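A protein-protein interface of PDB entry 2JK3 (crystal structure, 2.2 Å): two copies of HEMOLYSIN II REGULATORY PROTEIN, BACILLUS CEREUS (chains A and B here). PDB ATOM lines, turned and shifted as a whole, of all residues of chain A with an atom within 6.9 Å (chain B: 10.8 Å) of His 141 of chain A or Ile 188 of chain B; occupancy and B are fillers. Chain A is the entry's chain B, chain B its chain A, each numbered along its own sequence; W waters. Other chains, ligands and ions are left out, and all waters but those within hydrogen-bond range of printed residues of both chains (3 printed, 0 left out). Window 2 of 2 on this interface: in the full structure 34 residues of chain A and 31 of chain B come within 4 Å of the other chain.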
ATOM      1  N   GLY A 134      19.310 -20.026  18.667  1.00  0.00           N
ATOM      2  CA  GLY A 134      19.155 -20.322  20.099  1.00  0.00           C
ATOM      3  C   GLY A 134      18.963 -21.795  20.283  1.00  0.00           C
ATOM      4  O   GLY A 134      19.358 -22.372  21.281  1.00  0.00           O
ATOM      5  N   GLU A 135      18.300 -22.413  19.326  1.00  0.00           N
ATOM      6  CA  GLU A 135      18.157 -23.851  19.380  1.00  0.00           C
ATOM      7  C   GLU A 135      19.551 -24.515  19.350  1.00  0.00           C
ATOM      8  O   GLU A 135      19.871 -25.403  20.164  1.00  0.00           O
ATOM      9  CB  GLU A 135      17.325 -24.313  18.200  1.00  0.00           C
ATOM     10  CG  GLU A 135      17.161 -25.794  18.128  1.00  0.00           C
ATOM     11  CD  GLU A 135      16.159 -26.166  17.063  1.00  0.00           C
ATOM     12  OE1 GLU A 135      16.295 -25.633  15.938  1.00  0.00           O
ATOM     13  OE2 GLU A 135      15.228 -26.953  17.363  1.00  0.00           O
ATOM     14  N   GLN A 137      22.429 -23.300  20.102  1.00  0.00           N
ATOM     15  CA  GLN A 137      23.253 -23.010  21.282  1.00  0.00           C
ATOM     16  C   GLN A 137      22.643 -23.652  22.492  1.00  0.00           C
ATOM     17  O   GLN A 137      23.179 -23.547  23.589  1.00  0.00           O
ATOM     18  CB  GLN A 137      23.430 -21.528  21.503  1.00  0.00           C
ATOM     19  CG  GLN A 137      23.959 -20.872  20.283  1.00  0.00           C
ATOM     20  CD  GLN A 137      24.478 -19.501  20.590  1.00  0.00           C
ATOM     21  OE1 GLN A 137      24.547 -19.123  21.763  1.00  0.00           O
ATOM     22  NE2 GLN A 137      24.857 -18.731  19.542  1.00  0.00           N
ATOM     23  N   GLY A 138      21.511 -24.319  22.260  1.00  0.00           N
ATOM     24  CA  GLY A 138      20.839 -25.112  23.269  1.00  0.00           C
ATOM     25  C   GLY A 138      20.128 -24.304  24.339  1.00  0.00           C
ATOM     26  O   GLY A 138      19.798 -24.848  25.391  1.00  0.00           O
ATOM     27  N   VAL A 139      19.898 -23.011  24.075  1.00  0.00           N
ATOM     28  CA  VAL A 139      19.145 -22.140  24.999  1.00  0.00           C
ATOM     29  C   VAL A 139      17.639 -22.032  24.710  1.00  0.00           C
ATOM     30  O   VAL A 139      16.881 -21.562  25.559  1.00  0.00           O
ATOM     31  CB  VAL A 139      19.740 -20.744  25.021  1.00  0.00           C
ATOM     32  CG1 VAL A 139      21.119 -20.782  25.712  1.00  0.00           C
ATOM     33  CG2 VAL A 139      19.863 -20.210  23.552  1.00  0.00           C
ATOM     34  N   PHE A 140      17.183 -22.457  23.530  1.00  0.00           N
ATOM     35  CA  PHE A 140      15.755 -22.378  23.250  1.00  0.00           C
ATOM     36  C   PHE A 140      15.346 -23.769  22.875  1.00  0.00           C
ATOM     37  O   PHE A 140      16.047 -24.441  22.128  1.00  0.00           O
ATOM     38  CB  PHE A 140      15.426 -21.469  22.036  1.00  0.00           C
ATOM     39  CG  PHE A 140      15.694 -19.978  22.232  1.00  0.00           C
ATOM     40  CD1 PHE A 140      15.614 -19.371  23.471  1.00  0.00           C
ATOM     41  CD2 PHE A 140      15.968 -19.179  21.117  1.00  0.00           C
ATOM     42  CE1 PHE A 140      15.838 -17.971  23.607  1.00  0.00           C
ATOM     43  CE2 PHE A 140      16.201 -17.819  21.236  1.00  0.00           C
ATOM     44  CZ  PHE A 140      16.138 -17.211  22.506  1.00  0.00           C
ATOM     45  N   HIS A 141      14.182 -24.202  23.324  1.00  0.00           N
ATOM     46  CA  HIS A 141      13.776 -25.553  23.058  1.00  0.00           C
ATOM     47  C   HIS A 141      12.339 -25.559  22.519  1.00  0.00           C
ATOM     48  O   HIS A 141      11.436 -25.156  23.197  1.00  0.00           O
ATOM     49  CB  HIS A 141      13.901 -26.335  24.368  1.00  0.00           C
ATOM     50  CG  HIS A 141      15.241 -26.147  25.008  1.00  0.00           C
ATOM     51  ND1 HIS A 141      15.472 -25.209  25.998  1.00  0.00           N
ATOM     52  CD2 HIS A 141      16.444 -26.725  24.740  1.00  0.00           C
ATOM     53  CE1 HIS A 141      16.750 -25.243  26.339  1.00  0.00           C
ATOM     54  NE2 HIS A 141      17.360 -26.153  25.589  1.00  0.00           N
ATOM     55  N   PHE A 142      12.146 -26.066  21.313  1.00  0.00           N
ATOM     56  CA  PHE A 142      10.843 -26.101  20.714  1.00  0.00           C
ATOM     57  C   PHE A 142      10.852 -27.205  19.682  1.00  0.00           C
ATOM     58  O   PHE A 142      11.902 -27.548  19.117  1.00  0.00           O
ATOM     59  CB  PHE A 142      10.520 -24.740  20.069  1.00  0.00           C
ATOM     60  CG  PHE A 142      11.598 -24.223  19.141  1.00  0.00           C
ATOM     61  CD1 PHE A 142      11.726 -24.727  17.838  1.00  0.00           C
ATOM     62  CD2 PHE A 142      12.479 -23.231  19.556  1.00  0.00           C
ATOM     63  CE1 PHE A 142      12.715 -24.254  16.978  1.00  0.00           C
ATOM     64  CE2 PHE A 142      13.487 -22.756  18.696  1.00  0.00           C
ATOM     65  CZ  PHE A 142      13.611 -23.263  17.414  1.00  0.00           C
ATOM     66  N   PHE A 143       9.690 -27.775  19.430  1.00  0.00           N
ATOM     67  CA  PHE A 143       9.611 -28.873  18.498  1.00  0.00           C
ATOM     68  C   PHE A 143       9.659 -28.396  17.049  1.00  0.00           C
ATOM     69  O   PHE A 143      10.194 -29.045  16.170  1.00  0.00           O
ATOM     70  CB  PHE A 143       8.291 -29.605  18.690  1.00  0.00           C
ATOM     71  CG  PHE A 143       8.192 -30.840  17.882  1.00  0.00           C
ATOM     72  CD1 PHE A 143       8.752 -31.999  18.342  1.00  0.00           C
ATOM     73  CD2 PHE A 143       7.590 -30.828  16.632  1.00  0.00           C
ATOM     74  CE1 PHE A 143       8.700 -33.145  17.590  1.00  0.00           C
ATOM     75  CE2 PHE A 143       7.525 -31.982  15.890  1.00  0.00           C
ATOM     76  CZ  PHE A 143       8.081 -33.131  16.378  1.00  0.00           C
ATOM     77  N   SER A 144       9.006 -27.283  16.780  1.00  0.00           N
ATOM     78  CA  SER A 144       8.933 -26.805  15.419  1.00  0.00           C
ATOM     79  C   SER A 144       9.213 -25.325  15.304  1.00  0.00           C
ATOM     80  O   SER A 144       8.523 -24.504  15.913  1.00  0.00           O
ATOM     81  CB  SER A 144       7.586 -27.139  14.799  1.00  0.00           C
ATOM     82  OG  SER A 144       7.325 -26.257  13.720  1.00  0.00           O
ATOM     83  N   THR A 148       6.582 -22.325  16.167  1.00  0.00           N
ATOM     84  CA  THR A 148       7.006 -21.288  17.133  1.00  0.00           C
ATOM     85  C   THR A 148       6.939 -19.888  16.544  1.00  0.00           C
ATOM     86  O   THR A 148       6.540 -18.928  17.195  1.00  0.00           O
ATOM     87  CB  THR A 148       8.453 -21.560  17.589  1.00  0.00           C
ATOM     88  OG1 THR A 148       8.543 -22.925  18.019  1.00  0.00           O
ATOM     89  CG2 THR A 148       8.914 -20.596  18.701  1.00  0.00           C
ATOM     90  N   ALA A 181       9.038 -19.291  27.758  1.00  0.00           N
ATOM     91  CA  ALA A 181       8.393 -20.465  27.153  1.00  0.00           C
ATOM     92  C   ALA A 181       9.481 -21.249  26.423  1.00  0.00           C
ATOM     93  O   ALA A 181       9.570 -22.431  26.530  1.00  0.00           O
ATOM     94  CB  ALA A 181       7.276 -20.059  26.235  1.00  0.00           C
ATOM     95  N   LEU A 182      10.400 -20.542  25.784  1.00  0.00           N
ATOM     96  CA  LEU A 182      11.485 -21.158  25.018  1.00  0.00           C
ATOM     97  C   LEU A 182      12.665 -21.675  25.845  1.00  0.00           C
ATOM     98  O   LEU A 182      13.286 -22.695  25.497  1.00  0.00           O
ATOM     99  CB  LEU A 182      12.017 -20.104  24.047  1.00  0.00           C
ATOM    100  CG  LEU A 182      10.969 -19.574  23.089  1.00  0.00           C
ATOM    101  CD1 LEU A 182      11.565 -18.526  22.233  1.00  0.00           C
ATOM    102  CD2 LEU A 182      10.456 -20.749  22.200  1.00  0.00           C
ATOM    103  N   THR A 183      13.057 -20.934  26.879  1.00  0.00           N
ATOM    104  CA  THR A 183      14.201 -21.349  27.666  1.00  0.00           C
ATOM    105  C   THR A 183      13.754 -22.332  28.744  1.00  0.00           C
ATOM    106  O   THR A 183      14.587 -23.039  29.372  1.00  0.00           O
ATOM    107  CB  THR A 183      14.817 -20.163  28.404  1.00  0.00           C
ATOM    108  OG1 THR A 183      13.806 -19.603  29.242  1.00  0.00           O
ATOM    109  CG2 THR A 183      15.325 -19.109  27.441  1.00  0.00           C
ATOM    110  N   ASP A 184      12.442 -22.360  28.978  1.00  0.00           N
ATOM    111  CA  ASP A 184      11.863 -23.064  30.107  1.00  0.00           C
ATOM    112  C   ASP A 184      12.550 -22.646  31.408  1.00  0.00           C
ATOM    113  O   ASP A 184      12.704 -23.435  32.320  1.00  0.00           O
ATOM    114  CB  ASP A 184      11.998 -24.569  29.903  1.00  0.00           C
ATOM    115  CG  ASP A 184      11.024 -25.369  30.752  1.00  0.00           C
ATOM    116  OD1 ASP A 184       9.907 -24.872  31.066  1.00  0.00           O
ATOM    117  OD2 ASP A 184      11.374 -26.531  31.076  1.00  0.00           O
ATOM    118  N   LYS A 185      12.942 -21.392  31.516  1.00  0.00           N
ATOM    119  CA  LYS A 185      13.556 -20.942  32.762  1.00  0.00           C
ATOM    120  C   LYS A 185      13.021 -19.606  33.238  1.00  0.00           C
ATOM    121  O   LYS A 185      12.491 -18.836  32.463  1.00  0.00           O
ATOM    122  CB  LYS A 185      15.071 -20.863  32.587  1.00  0.00           C
ATOM    123  CG  LYS A 185      15.726 -22.226  32.374  1.00  0.00           C
ATOM    124  CD  LYS A 185      17.157 -22.046  31.885  1.00  0.00           C
ATOM    125  CE  LYS A 185      18.065 -23.006  32.596  1.00  0.00           C
ATOM    126  NZ  LYS A 185      19.213 -22.248  33.128  1.00  0.00           N
ATOM    127  N   HIS B 141       4.587 -30.230  28.813  1.00  0.00           N
ATOM    128  CA  HIS B 141       5.648 -29.528  29.539  1.00  0.00           C
ATOM    129  C   HIS B 141       5.540 -28.126  29.078  1.00  0.00           C
ATOM    130  O   HIS B 141       5.504 -27.854  27.855  1.00  0.00           O
ATOM    131  CB  HIS B 141       7.016 -30.107  29.182  1.00  0.00           C
ATOM    132  CG  HIS B 141       7.063 -31.602  29.292  1.00  0.00           C
ATOM    133  ND1 HIS B 141       7.512 -32.253  30.425  1.00  0.00           N
ATOM    134  CD2 HIS B 141       6.671 -32.573  28.431  1.00  0.00           C
ATOM    135  CE1 HIS B 141       7.412 -33.560  30.248  1.00  0.00           C
ATOM    136  NE2 HIS B 141       6.891 -33.782  29.050  1.00  0.00           N
ATOM    137  N   PHE B 142       5.359 -27.222  30.031  1.00  0.00           N
ATOM    138  CA  PHE B 142       5.387 -25.846  29.651  1.00  0.00           C
ATOM    139  C   PHE B 142       5.820 -25.102  30.892  1.00  0.00           C
ATOM    140  O   PHE B 142       5.756 -25.623  32.014  1.00  0.00           O
ATOM    141  CB  PHE B 142       4.037 -25.347  29.146  1.00  0.00           C
ATOM    142  CG  PHE B 142       2.859 -25.857  29.964  1.00  0.00           C
ATOM    143  CD1 PHE B 142       2.569 -25.315  31.210  1.00  0.00           C
ATOM    144  CD2 PHE B 142       2.071 -26.899  29.490  1.00  0.00           C
ATOM    145  CE1 PHE B 142       1.507 -25.801  31.955  1.00  0.00           C
ATOM    146  CE2 PHE B 142       0.994 -27.388  30.228  1.00  0.00           C
ATOM    147  CZ  PHE B 142       0.700 -26.849  31.438  1.00  0.00           C
ATOM    148  N   PHE B 143       6.247 -23.883  30.702  1.00  0.00           N
ATOM    149  CA  PHE B 143       6.684 -23.113  31.860  1.00  0.00           C
ATOM    150  C   PHE B 143       5.540 -22.399  32.644  1.00  0.00           C
ATOM    151  O   PHE B 143       5.618 -22.239  33.900  1.00  0.00           O
ATOM    152  CB  PHE B 143       7.725 -22.108  31.413  1.00  0.00           C
ATOM    153  CG  PHE B 143       8.323 -21.327  32.560  1.00  0.00           C
ATOM    154  CD1 PHE B 143       9.392 -21.826  33.271  1.00  0.00           C
ATOM    155  CD2 PHE B 143       7.769 -20.121  32.944  1.00  0.00           C
ATOM    156  CE1 PHE B 143       9.928 -21.105  34.360  1.00  0.00           C
ATOM    157  CE2 PHE B 143       8.335 -19.375  34.054  1.00  0.00           C
ATOM    158  CZ  PHE B 143       9.378 -19.889  34.719  1.00  0.00           C
ATOM    159  N   HIS B 147       0.561 -18.461  29.989  1.00  0.00           N
ATOM    160  CA  HIS B 147       1.201 -18.233  28.669  1.00  0.00           C
ATOM    161  C   HIS B 147       0.690 -19.242  27.636  1.00  0.00           C
ATOM    162  O   HIS B 147       0.353 -18.906  26.493  1.00  0.00           O
ATOM    163  CB  HIS B 147       2.752 -18.229  28.728  1.00  0.00           C
ATOM    164  CG  HIS B 147       3.373 -18.148  27.362  1.00  0.00           C
ATOM    165  ND1 HIS B 147       3.444 -16.962  26.653  1.00  0.00           N
ATOM    166  CD2 HIS B 147       3.823 -19.117  26.518  1.00  0.00           C
ATOM    167  CE1 HIS B 147       3.956 -17.198  25.456  1.00  0.00           C
ATOM    168  NE2 HIS B 147       4.221 -18.490  25.358  1.00  0.00           N
ATOM    169  N   TRP B 151      -1.268 -18.578  23.961  1.00  0.00           N
ATOM    170  CA  TRP B 151      -0.852 -18.793  22.580  1.00  0.00           C
ATOM    171  C   TRP B 151      -1.721 -19.793  21.911  1.00  0.00           C
ATOM    172  O   TRP B 151      -1.900 -19.741  20.689  1.00  0.00           O
ATOM    173  CB  TRP B 151       0.655 -19.106  22.398  1.00  0.00           C
ATOM    174  CG  TRP B 151       1.215 -20.393  22.906  1.00  0.00           C
ATOM    175  CD1 TRP B 151       2.003 -20.593  24.066  1.00  0.00           C
ATOM    176  CD2 TRP B 151       1.141 -21.666  22.249  1.00  0.00           C
ATOM    177  NE1 TRP B 151       2.335 -21.936  24.153  1.00  0.00           N
ATOM    178  CE2 TRP B 151       1.809 -22.610  23.064  1.00  0.00           C
ATOM    179  CE3 TRP B 151       0.490 -22.119  21.074  1.00  0.00           C
ATOM    180  CZ2 TRP B 151       1.943 -23.975  22.680  1.00  0.00           C
ATOM    181  CZ3 TRP B 151       0.562 -23.448  20.743  1.00  0.00           C
ATOM    182  CH2 TRP B 151       1.285 -24.374  21.546  1.00  0.00           C
ATOM    183  N   SER B 180       2.509 -31.598  19.470  1.00  0.00           N
ATOM    184  CA  SER B 180       3.956 -31.763  19.418  1.00  0.00           C
ATOM    185  C   SER B 180       4.650 -30.649  20.195  1.00  0.00           C
ATOM    186  O   SER B 180       5.595 -30.907  20.890  1.00  0.00           O
ATOM    187  CB  SER B 180       4.477 -31.855  17.998  1.00  0.00           C
ATOM    188  OG  SER B 180       4.272 -30.678  17.264  1.00  0.00           O
ATOM    189  N   ALA B 181       4.150 -29.419  20.133  1.00  0.00           N
ATOM    190  CA  ALA B 181       4.745 -28.353  20.961  1.00  0.00           C
ATOM    191  C   ALA B 181       4.670 -28.664  22.450  1.00  0.00           C
ATOM    192  O   ALA B 181       5.639 -28.445  23.186  1.00  0.00           O
ATOM    193  CB  ALA B 181       4.104 -27.037  20.693  1.00  0.00           C
ATOM    194  N   LEU B 182       3.541 -29.168  22.919  1.00  0.00           N
ATOM    195  CA  LEU B 182       3.377 -29.390  24.371  1.00  0.00           C
ATOM    196  C   LEU B 182       4.098 -30.621  24.932  1.00  0.00           C
ATOM    197  O   LEU B 182       4.622 -30.590  26.061  1.00  0.00           O
ATOM    198  CB  LEU B 182       1.891 -29.534  24.700  1.00  0.00           C
ATOM    199  CG  LEU B 182       1.030 -28.315  24.365  1.00  0.00           C
ATOM    200  CD1 LEU B 182      -0.434 -28.657  24.378  1.00  0.00           C
ATOM    201  CD2 LEU B 182       1.304 -27.296  25.346  1.00  0.00           C
ATOM    202  N   THR B 183       4.116 -31.701  24.159  1.00  0.00           N
ATOM    203  CA  THR B 183       4.743 -32.957  24.592  1.00  0.00           C
ATOM    204  C   THR B 183       6.262 -32.945  24.473  1.00  0.00           C
ATOM    205  O   THR B 183       6.932 -33.740  25.085  1.00  0.00           O
ATOM    206  CB  THR B 183       4.234 -34.164  23.784  1.00  0.00           C
ATOM    207  OG1 THR B 183       4.519 -33.952  22.415  1.00  0.00           O
ATOM    208  CG2 THR B 183       2.740 -34.358  23.944  1.00  0.00           C
ATOM    209  N   ASP B 184       6.813 -32.059  23.666  1.00  0.00           N
ATOM    210  CA  ASP B 184       8.267 -31.984  23.558  1.00  0.00           C
ATOM    211  C   ASP B 184       8.866 -31.673  24.924  1.00  0.00           C
ATOM    212  O   ASP B 184       8.503 -30.681  25.526  1.00  0.00           O
ATOM    213  CB  ASP B 184       8.660 -30.870  22.589  1.00  0.00           C
ATOM    214  CG  ASP B 184      10.159 -30.825  22.338  1.00  0.00           C
ATOM    215  OD1 ASP B 184      10.714 -31.841  21.893  1.00  0.00           O
ATOM    216  OD2 ASP B 184      10.788 -29.787  22.589  1.00  0.00           O
ATOM    217  N   LYS B 185       9.779 -32.498  25.419  1.00  0.00           N
ATOM    218  CA  LYS B 185      10.411 -32.209  26.703  1.00  0.00           C
ATOM    219  C   LYS B 185      11.808 -31.639  26.531  1.00  0.00           C
ATOM    220  O   LYS B 185      12.669 -32.276  25.941  1.00  0.00           O
ATOM    221  CB  LYS B 185      10.497 -33.458  27.590  1.00  0.00           C
ATOM    222  CG  LYS B 185      10.712 -33.071  29.034  1.00  0.00           C
ATOM    223  CD  LYS B 185      10.805 -34.247  29.998  1.00  0.00           C
ATOM    224  CE  LYS B 185      11.318 -33.738  31.350  1.00  0.00           C
ATOM    225  NZ  LYS B 185      11.289 -34.740  32.449  1.00  0.00           N
ATOM    226  N   PRO B 186      12.047 -30.442  27.079  1.00  0.00           N
ATOM    227  CA  PRO B 186      13.332 -29.762  26.861  1.00  0.00           C
ATOM    228  C   PRO B 186      14.491 -30.626  27.326  1.00  0.00           C
ATOM    229  O   PRO B 186      14.386 -31.320  28.349  1.00  0.00           O
ATOM    230  CB  PRO B 186      13.224 -28.472  27.717  1.00  0.00           C
ATOM    231  CG  PRO B 186      11.726 -28.215  27.821  1.00  0.00           C
ATOM    232  CD  PRO B 186      11.112 -29.637  27.888  1.00  0.00           C
ATOM    233  N   ASN B 187      15.573 -30.605  26.563  1.00  0.00           N
ATOM    234  CA  ASN B 187      16.762 -31.318  26.981  1.00  0.00           C
ATOM    235  C   ASN B 187      17.171 -31.034  28.443  1.00  0.00           C
ATOM    236  O   ASN B 187      17.055 -31.913  29.309  1.00  0.00           O
ATOM    237  CB  ASN B 187      17.913 -31.053  26.023  1.00  0.00           C
ATOM    238  CG  ASN B 187      18.765 -32.271  25.824  1.00  0.00           C
ATOM    239  OD1 ASN B 187      18.480 -33.328  26.396  1.00  0.00           O
ATOM    240  ND2 ASN B 187      19.816 -32.143  25.014  1.00  0.00           N
ATOM    241  N   ILE B 188      17.621 -29.818  28.734  1.00  0.00           N
ATOM    242  CA  ILE B 188      17.987 -29.470  30.116  1.00  0.00           C
ATOM    243  C   ILE B 188      17.870 -30.662  31.081  1.00  0.00           C
ATOM    244  O   ILE B 188      18.319 -30.593  32.223  1.00  0.00           O
ATOM    245  CB  ILE B 188      17.130 -28.303  30.662  1.00  0.00           C
ATOM    246  CG1 ILE B 188      15.642 -28.674  30.642  1.00  0.00           C
ATOM    247  CG2 ILE B 188      17.353 -27.057  29.835  1.00  0.00           C
ATOM    248  CD1 ILE B 188      14.691 -27.542  31.081  1.00  0.00           C
HETATM  249  O   HOH W   1      13.215 -30.105  20.535  1.00  0.00           O
HETATM  250  O   HOH W   2       9.819 -27.840  24.034  1.00  0.00           O
HETATM  251  O   HOH W   3       7.926 -27.260  22.026  1.00  0.00           O
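Water W2 lies within hydrogen-bond range of the side-chain carboxylate (OD2) of Asp 184 of chain B and the backbone carbonyl oxygen (O) of His 141 of chain A. Water W3 bridges the backbone carbonyl oxygen of Ala 181 of chain B (2.8 Å) and the backbone NH of Phe 143 of chain A (3.2 Å). Water W1 bridges the side-chain carboxylate of Asp 184 of chain B (3.2 Å) and the backbone carbonyl oxygen of Phe 142 of chain A (3.2 Å).
No residue of chain B comes within 4 Å of Gly 138 of chain A. Printed residues of chain B within 4 Å of His 141 of chain A: Ile 188 (3.98 Å). Of chain B, only Asp 184 comes within 4 Å of Phe 142 of chain A. Printed residues of chain B within 4 Å of Phe 143 of chain A: Ser 180 and Asp 184. Printed residues of chain B within 4 Å of Ala 181 of chain A: His 147. Of chain B, only Phe 143 (3.5 Å), Pro 186 (3.7 Å) and Ile 188 (3.5 Å) come within 4 Å of Asp 184 of chain A. Of the printed residues of chain B, Lys 185 of chain A touches Phe 143. Of the printed residues of chain A, His 147 of chain B touches Ala 181. Of the printed residues of chain A, Asp 184 of chain B touches Phe 142 (3.9 Å) and Phe 143 (3.9 Å). Of the printed residues of chain A, Ile 188 of chain B touches His 141 and Asp 184. The nearest printed residue of chain B that does not touch His 141 of chain A is Pro 186 of chain B (4.03 Å). The nearest printed residue of chain A that does not touch Ile 188 of chain B is Thr 183 of chain A (4.8 Å).
A ring nitrogen (NE2) of His 141 of chain A is in hydrogen-bond range of the backbone carbonyl oxygen (O) of Gly 138 of chain A, 2.8 Å away. O of Leu 182 of chain A lies within hydrogen-bond range of N of His 141 of chain A. OG1 of Thr 183 of chain A lies within hydrogen-bond range of N of Lys 185 of chain A.
Printed residues of chain B that touch a printed residue of chain A: Phe 143, His 147, Ser 180, Asp 184, Pro 186 and Ile 188. Along chain B the printed residues that touch a printed residue of chain A span positions 143 to 188. Hydrophobic or aromatic side chains of chain A within 4 Å of the printed part of chain B: His 141, Phe 143 and Ala 181. Among the printed residues, 9 pairs touch across the chains.
Ile 188 of chain B touches His 141 of chain A (CG2 to CE1, 3.98 Å). Phe 142 of chain A touches Asp 184 of chain B (C to OD2, 3.9 Å). Phe 143 of chain A touches Ser 180 of chain B (CD2 to OG, 3.4 Å). Phe 143 of chain A touches Asp 184 of chain B (N to OD2, 3.9 Å). Ala 181 of chain A touches His 147 of chain B. Phe 143 of chain B touches Asp 184 of chain A. Asp 184 of chain A touches Pro 186 of chain B (OD2 to CG, 3.7 Å). Asp 184 of chain A touches Ile 188 of chain B (OD2 to CD1, 3.5 Å). Lys 185 of chain A touches Phe 143 of chain B.
Phe 142 of chain A touches Asp 184 of chain B, but with the chains exchanged Asp 184 of chain A does not touch Phe 142 of chain B (4.1 Å). Phe 143 of chain A touches Asp 184 of chain B, and with the chains exchanged Asp 184 of chain A touches Phe 143 of chain B. Lys 185 of chain A touches Phe 143 of chain B, but with the chains exchanged Phe 143 of chain A does not touch Lys 185 of chain B (7.2 Å). Positions printed for both chains: 141, 142, 143, 181, 182, 183, 184 and 185.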
